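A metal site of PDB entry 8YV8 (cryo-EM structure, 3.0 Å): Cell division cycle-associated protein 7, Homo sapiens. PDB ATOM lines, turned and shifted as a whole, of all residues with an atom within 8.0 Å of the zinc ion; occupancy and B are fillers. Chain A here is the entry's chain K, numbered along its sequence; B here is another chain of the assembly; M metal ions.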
ATOM      1  N   THR A   6      -8.789 -18.936   5.071  1.00  0.00           N
ATOM      2  CA  THR A   6      -8.410 -18.982   6.478  1.00  0.00           C
ATOM      3  C   THR A   6      -6.929 -19.306   6.600  1.00  0.00           C
ATOM      4  O   THR A   6      -6.474 -20.331   6.082  1.00  0.00           O
ATOM      5  CB  THR A   6      -9.252 -20.007   7.247  1.00  0.00           C
ATOM      6  OG1 THR A   6      -9.337 -21.210   6.487  1.00  0.00           O
ATOM      7  CG2 THR A   6     -10.648 -19.463   7.493  1.00  0.00           C
ATOM      8  N   CYS A   7      -6.195 -18.453   7.292  1.00  0.00           N
ATOM      9  CA  CYS A   7      -4.765 -18.671   7.497  1.00  0.00           C
ATOM     10  C   CYS A   7      -4.553 -19.823   8.467  1.00  0.00           C
ATOM     11  O   CYS A   7      -5.382 -20.106   9.333  1.00  0.00           O
ATOM     12  CB  CYS A   7      -4.110 -17.400   8.034  1.00  0.00           C
ATOM     13  SG  CYS A   7      -2.453 -17.627   8.711  1.00  0.00           S
ATOM     14  N   HIS A   8      -3.418 -20.509   8.309  1.00  0.00           N
ATOM     15  CA  HIS A   8      -3.127 -21.635   9.194  1.00  0.00           C
ATOM     16  C   HIS A   8      -2.701 -21.154  10.572  1.00  0.00           C
ATOM     17  O   HIS A   8      -3.128 -21.719  11.594  1.00  0.00           O
ATOM     18  CB  HIS A   8      -2.039 -22.517   8.570  1.00  0.00           C
ATOM     19  CG  HIS A   8      -1.526 -23.588   9.480  1.00  0.00           C
ATOM     20  ND1 HIS A   8      -2.184 -24.793   9.655  1.00  0.00           N
ATOM     21  CD2 HIS A   8      -0.428 -23.644  10.264  1.00  0.00           C
ATOM     22  CE1 HIS A   8      -1.510 -25.535  10.510  1.00  0.00           C
ATOM     23  NE2 HIS A   8      -0.434 -24.867  10.890  1.00  0.00           N
ATOM     24  N   GLN A   9      -1.869 -20.112  10.636  1.00  0.00           N
ATOM     25  CA  GLN A   9      -1.379 -19.631  11.927  1.00  0.00           C
ATOM     26  C   GLN A   9      -2.476 -18.933  12.717  1.00  0.00           C
ATOM     27  O   GLN A   9      -2.698 -19.223  13.892  1.00  0.00           O
ATOM     28  CB  GLN A   9      -0.194 -18.698  11.717  1.00  0.00           C
ATOM     29  N   CYS A  10      -3.194 -17.998  12.078  1.00  0.00           N
ATOM     30  CA  CYS A  10      -4.178 -17.189  12.793  1.00  0.00           C
ATOM     31  C   CYS A  10      -5.559 -17.809  12.792  1.00  0.00           C
ATOM     32  O   CYS A  10      -6.359 -17.503  13.680  1.00  0.00           O
ATOM     33  CB  CYS A  10      -4.239 -15.787  12.185  1.00  0.00           C
ATOM     34  SG  CYS A  10      -5.093 -15.705  10.599  1.00  0.00           S
ATOM     35  N   ARG A  11      -5.865 -18.666  11.814  1.00  0.00           N
ATOM     36  CA  ARG A  11      -7.099 -19.455  11.792  1.00  0.00           C
ATOM     37  C   ARG A  11      -8.343 -18.579  11.805  1.00  0.00           C
ATOM     38  O   ARG A  11      -9.361 -18.934  12.416  1.00  0.00           O
ATOM     39  CB  ARG A  11      -7.108 -20.471  12.931  1.00  0.00           C
ATOM     40  CG  ARG A  11      -7.992 -21.681  12.716  1.00  0.00           C
ATOM     41  CD  ARG A  11      -7.705 -22.768  13.732  1.00  0.00           C
ATOM     42  NE  ARG A  11      -6.411 -22.577  14.389  1.00  0.00           N
ATOM     43  CZ  ARG A  11      -6.267 -22.270  15.670  1.00  0.00           C
ATOM     44  NH1 ARG A  11      -7.305 -22.106  16.468  1.00  0.00           N
ATOM     45  NH2 ARG A  11      -5.035 -22.126  16.157  1.00  0.00           N
ATOM     46  N   GLN A  12      -8.290 -17.424  11.158  1.00  0.00           N
ATOM     47  CA  GLN A  12      -9.418 -16.521  11.033  1.00  0.00           C
ATOM     48  C   GLN A  12      -9.826 -16.386   9.568  1.00  0.00           C
ATOM     49  O   GLN A  12      -9.090 -16.772   8.650  1.00  0.00           O
ATOM     50  CB  GLN A  12      -9.086 -15.154  11.628  1.00  0.00           C
ATOM     51  CG  GLN A  12      -8.905 -15.152  13.140  1.00  0.00           C
ATOM     52  CD  GLN A  12     -10.226 -15.197  13.891  1.00  0.00           C
ATOM     53  OE1 GLN A  12     -11.151 -15.905  13.508  1.00  0.00           O
ATOM     54  NE2 GLN A  12     -10.317 -14.428  14.967  1.00  0.00           N
ATOM     55  N   THR A  14     -10.622 -13.876   6.556  1.00  0.00           N
ATOM     56  CA  THR A  14     -10.382 -12.528   6.078  1.00  0.00           C
ATOM     57  C   THR A  14     -10.145 -12.575   4.571  1.00  0.00           C
ATOM     58  O   THR A  14      -9.804 -13.622   4.015  1.00  0.00           O
ATOM     59  CB  THR A  14      -9.182 -11.871   6.781  1.00  0.00           C
ATOM     60  OG1 THR A  14      -9.137 -12.303   8.153  1.00  0.00           O
ATOM     61  CG2 THR A  14      -9.287 -10.354   6.741  1.00  0.00           C
ATOM     62  N   ASP A  16      -7.832 -11.757   1.875  1.00  0.00           N
ATOM     63  CA  ASP A  16      -6.431 -11.436   1.607  1.00  0.00           C
ATOM     64  C   ASP A  16      -5.807 -12.572   0.818  1.00  0.00           C
ATOM     65  O   ASP A  16      -6.229 -13.735   0.934  1.00  0.00           O
ATOM     66  CB  ASP A  16      -5.648 -11.215   2.905  1.00  0.00           C
ATOM     67  CG  ASP A  16      -5.472 -12.487   3.703  1.00  0.00           C
ATOM     68  OD1 ASP A  16      -6.475 -12.991   4.253  1.00  0.00           O
ATOM     69  OD2 ASP A  16      -4.329 -12.993   3.767  1.00  0.00           O
ATOM     70  N   GLN A  32      -1.399 -22.788   3.526  1.00  0.00           N
ATOM     71  CA  GLN A  32      -1.872 -21.425   3.306  1.00  0.00           C
ATOM     72  C   GLN A  32      -1.610 -20.582   4.554  1.00  0.00           C
ATOM     73  O   GLN A  32      -2.011 -20.962   5.656  1.00  0.00           O
ATOM     74  CB  GLN A  32      -3.360 -21.412   2.976  1.00  0.00           C
ATOM     75  CG  GLN A  32      -3.704 -22.108   1.663  1.00  0.00           C
ATOM     76  CD  GLN A  32      -5.116 -21.811   1.208  1.00  0.00           C
ATOM     77  OE1 GLN A  32      -5.959 -21.366   1.995  1.00  0.00           O
ATOM     78  NE2 GLN A  32      -5.386 -22.051  -0.068  1.00  0.00           N
ATOM     79  N   PHE A  33      -0.937 -19.448   4.367  1.00  0.00           N
ATOM     80  CA  PHE A  33      -0.636 -18.525   5.444  1.00  0.00           C
ATOM     81  C   PHE A  33      -0.938 -17.104   5.004  1.00  0.00           C
ATOM     82  O   PHE A  33      -0.803 -16.775   3.822  1.00  0.00           O
ATOM     83  CB  PHE A  33       0.822 -18.622   5.888  1.00  0.00           C
ATOM     84  CG  PHE A  33       1.095 -19.718   6.866  1.00  0.00           C
ATOM     85  CD1 PHE A  33       1.213 -21.030   6.439  1.00  0.00           C
ATOM     86  CD2 PHE A  33       1.236 -19.446   8.219  1.00  0.00           C
ATOM     87  CE1 PHE A  33       1.461 -22.045   7.333  1.00  0.00           C
ATOM     88  CE2 PHE A  33       1.482 -20.452   9.117  1.00  0.00           C
ATOM     89  CZ  PHE A  33       1.600 -21.760   8.681  1.00  0.00           C
ATOM     90  N   CYS A  34      -1.331 -16.271   5.954  1.00  0.00           N
ATOM     91  CA  CYS A  34      -1.621 -14.875   5.691  1.00  0.00           C
ATOM     92  C   CYS A  34      -0.413 -14.007   6.030  1.00  0.00           C
ATOM     93  O   CYS A  34       0.389 -14.348   6.897  1.00  0.00           O
ATOM     94  CB  CYS A  34      -2.830 -14.402   6.489  1.00  0.00           C
ATOM     95  SG  CYS A  34      -2.537 -14.305   8.264  1.00  0.00           S
ATOM     96  N   GLY A  35      -0.295 -12.888   5.324  1.00  0.00           N
ATOM     97  CA  GLY A  35       0.805 -11.971   5.481  1.00  0.00           C
ATOM     98  C   GLY A  35       1.073 -11.492   6.897  1.00  0.00           C
ATOM     99  O   GLY A  35       2.207 -11.530   7.379  1.00  0.00           O
ATOM    100  N   PRO A  36       0.031 -11.026   7.608  1.00  0.00           N
ATOM    101  CA  PRO A  36       0.252 -10.534   8.973  1.00  0.00           C
ATOM    102  C   PRO A  36       0.856 -11.560   9.908  1.00  0.00           C
ATOM    103  O   PRO A  36       1.611 -11.194  10.819  1.00  0.00           O
ATOM    104  CB  PRO A  36      -1.159 -10.119   9.433  1.00  0.00           C
ATOM    105  CG  PRO A  36      -1.865  -9.793   8.172  1.00  0.00           C
ATOM    106  CD  PRO A  36      -1.346 -10.755   7.153  1.00  0.00           C
ATOM    107  N   CYS A  37       0.572 -12.850   9.699  1.00  0.00           N
ATOM    108  CA  CYS A  37       1.119 -13.865  10.583  1.00  0.00           C
ATOM    109  C   CYS A  37       2.551 -14.228  10.193  1.00  0.00           C
ATOM    110  O   CYS A  37       3.449 -14.256  11.050  1.00  0.00           O
ATOM    111  CB  CYS A  37       0.225 -15.109  10.573  1.00  0.00           C
ATOM    112  SG  CYS A  37      -1.308 -14.928  11.527  1.00  0.00           S
ATOM    113  N   LEU A  38       2.800 -14.495   8.913  1.00  0.00           N
ATOM    114  CA  LEU A  38       4.127 -14.946   8.509  1.00  0.00           C
ATOM    115  C   LEU A  38       5.156 -13.821   8.599  1.00  0.00           C
ATOM    116  O   LEU A  38       6.319 -14.080   8.941  1.00  0.00           O
ATOM    117  CB  LEU A  38       4.088 -15.551   7.096  1.00  0.00           C
ATOM    118  CG  LEU A  38       3.330 -14.905   5.924  1.00  0.00           C
ATOM    119  CD1 LEU A  38       3.988 -13.636   5.424  1.00  0.00           C
ATOM    120  CD2 LEU A  38       3.175 -15.916   4.798  1.00  0.00           C
ATOM    121  P    DT B  14       0.487 -13.065  17.938  1.00  0.00           P
ATOM    122  OP1  DT B  14       1.894 -13.103  18.374  1.00  0.00           O
ATOM    123  OP2  DT B  14       0.113 -13.589  16.608  1.00  0.00           O
ATOM    124  O5'  DT B  14      -0.417 -13.811  19.019  1.00  0.00           O
ATOM    125  C5'  DT B  14      -0.775 -15.169  18.841  1.00  0.00           C
ATOM    126  C4'  DT B  14      -1.753 -15.615  19.899  1.00  0.00           C
ATOM    127  O4'  DT B  14      -2.973 -14.838  19.798  1.00  0.00           O
ATOM    128  C3'  DT B  14      -2.181 -17.089  19.806  1.00  0.00           C
ATOM    129  O3'  DT B  14      -2.044 -17.720  21.073  1.00  0.00           O
ATOM    130  C2'  DT B  14      -3.638 -17.005  19.367  1.00  0.00           C
ATOM    131  C1'  DT B  14      -4.068 -15.687  19.975  1.00  0.00           C
ATOM    132  N1   DT B  14      -5.261 -15.100  19.313  1.00  0.00           N
ATOM    133  C2   DT B  14      -6.510 -15.364  19.826  1.00  0.00           C
ATOM    134  O2   DT B  14      -6.696 -16.044  20.812  1.00  0.00           O
ATOM    135  N3   DT B  14      -7.547 -14.776  19.149  1.00  0.00           N
ATOM    136  C4   DT B  14      -7.456 -13.981  18.016  1.00  0.00           C
ATOM    137  O4   DT B  14      -8.440 -13.502  17.477  1.00  0.00           O
ATOM    138  C5   DT B  14      -6.112 -13.749  17.524  1.00  0.00           C
ATOM    139  C7   DT B  14      -5.898 -12.896  16.312  1.00  0.00           C
ATOM    140  C6   DT B  14      -5.097 -14.314  18.189  1.00  0.00           C
ATOM    141  N1  5CM B  15      -7.122 -19.630  20.052  1.00  0.00           N
ATOM    142  C2  5CM B  15      -8.351 -19.156  20.058  1.00  0.00           C
ATOM    143  N3  5CM B  15      -8.833 -18.451  19.048  1.00  0.00           N
ATOM    144  C4  5CM B  15      -8.072 -18.221  17.997  1.00  0.00           C
ATOM    145  C5  5CM B  15      -6.775 -18.706  17.955  1.00  0.00           C
ATOM    146  C5A 5CM B  15      -5.878 -18.437  16.751  1.00  0.00           C
ATOM    147  C6  5CM B  15      -6.309 -19.431  19.044  1.00  0.00           C
ATOM    148  O2  5CM B  15      -9.050 -19.359  20.990  1.00  0.00           O
ATOM    149  N4  5CM B  15      -8.584 -17.451  16.884  1.00  0.00           N
ATOM    150  C1' 5CM B  15      -6.679 -20.398  21.219  1.00  0.00           C
ATOM    151  C2' 5CM B  15      -5.807 -21.259  20.886  1.00  0.00           C
ATOM    152  C3' 5CM B  15      -4.797 -21.287  21.993  1.00  0.00           C
ATOM    153  C4' 5CM B  15      -5.079 -20.017  22.872  1.00  0.00           C
ATOM    154  O4' 5CM B  15      -5.992 -19.403  22.301  1.00  0.00           O
ATOM    155  O3' 5CM B  15      -4.787 -22.511  22.652  1.00  0.00           O
ATOM    156  C5' 5CM B  15      -3.812 -19.062  22.943  1.00  0.00           C
ATOM    157  O5' 5CM B  15      -2.657 -19.745  22.553  1.00  0.00           O
ATOM    158  P   5CM B  15      -1.889 -19.314  21.156  1.00  0.00           P
ATOM    159  OP1 5CM B  15      -0.432 -19.675  21.203  1.00  0.00           O
ATOM    160  OP2 5CM B  15      -2.556 -19.952  19.959  1.00  0.00           O
HETATM  161 ZN    ZN M   1      -2.849 -15.696   9.977  1.00  0.00          ZN
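SG of Cys 34 binds the zinc ion, 2.2 Å away. SG of Cys 37 is bound to the zinc ion (2.3 Å). The side-chain sulfur (SG) of Cys 10 binds the zinc ion. SG of Cys 7 is bound to the zinc ion, at 2.3 Å.
Within 4 Å of the zinc ion: Cys 7, Cys 10, Cys 34 and Cys 37. Along chain A the residues within 4 Å of the zinc ion span positions 7 to 37.
The side-chain sulfur (SG) of Cys 10 sits close to the backbone NH (N) of Gln 12 (3.7 Å). The side-chain sulfur (SG) of Cys 7 lies close to the backbone NH (N) of Gln 9, 3.2 Å away.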
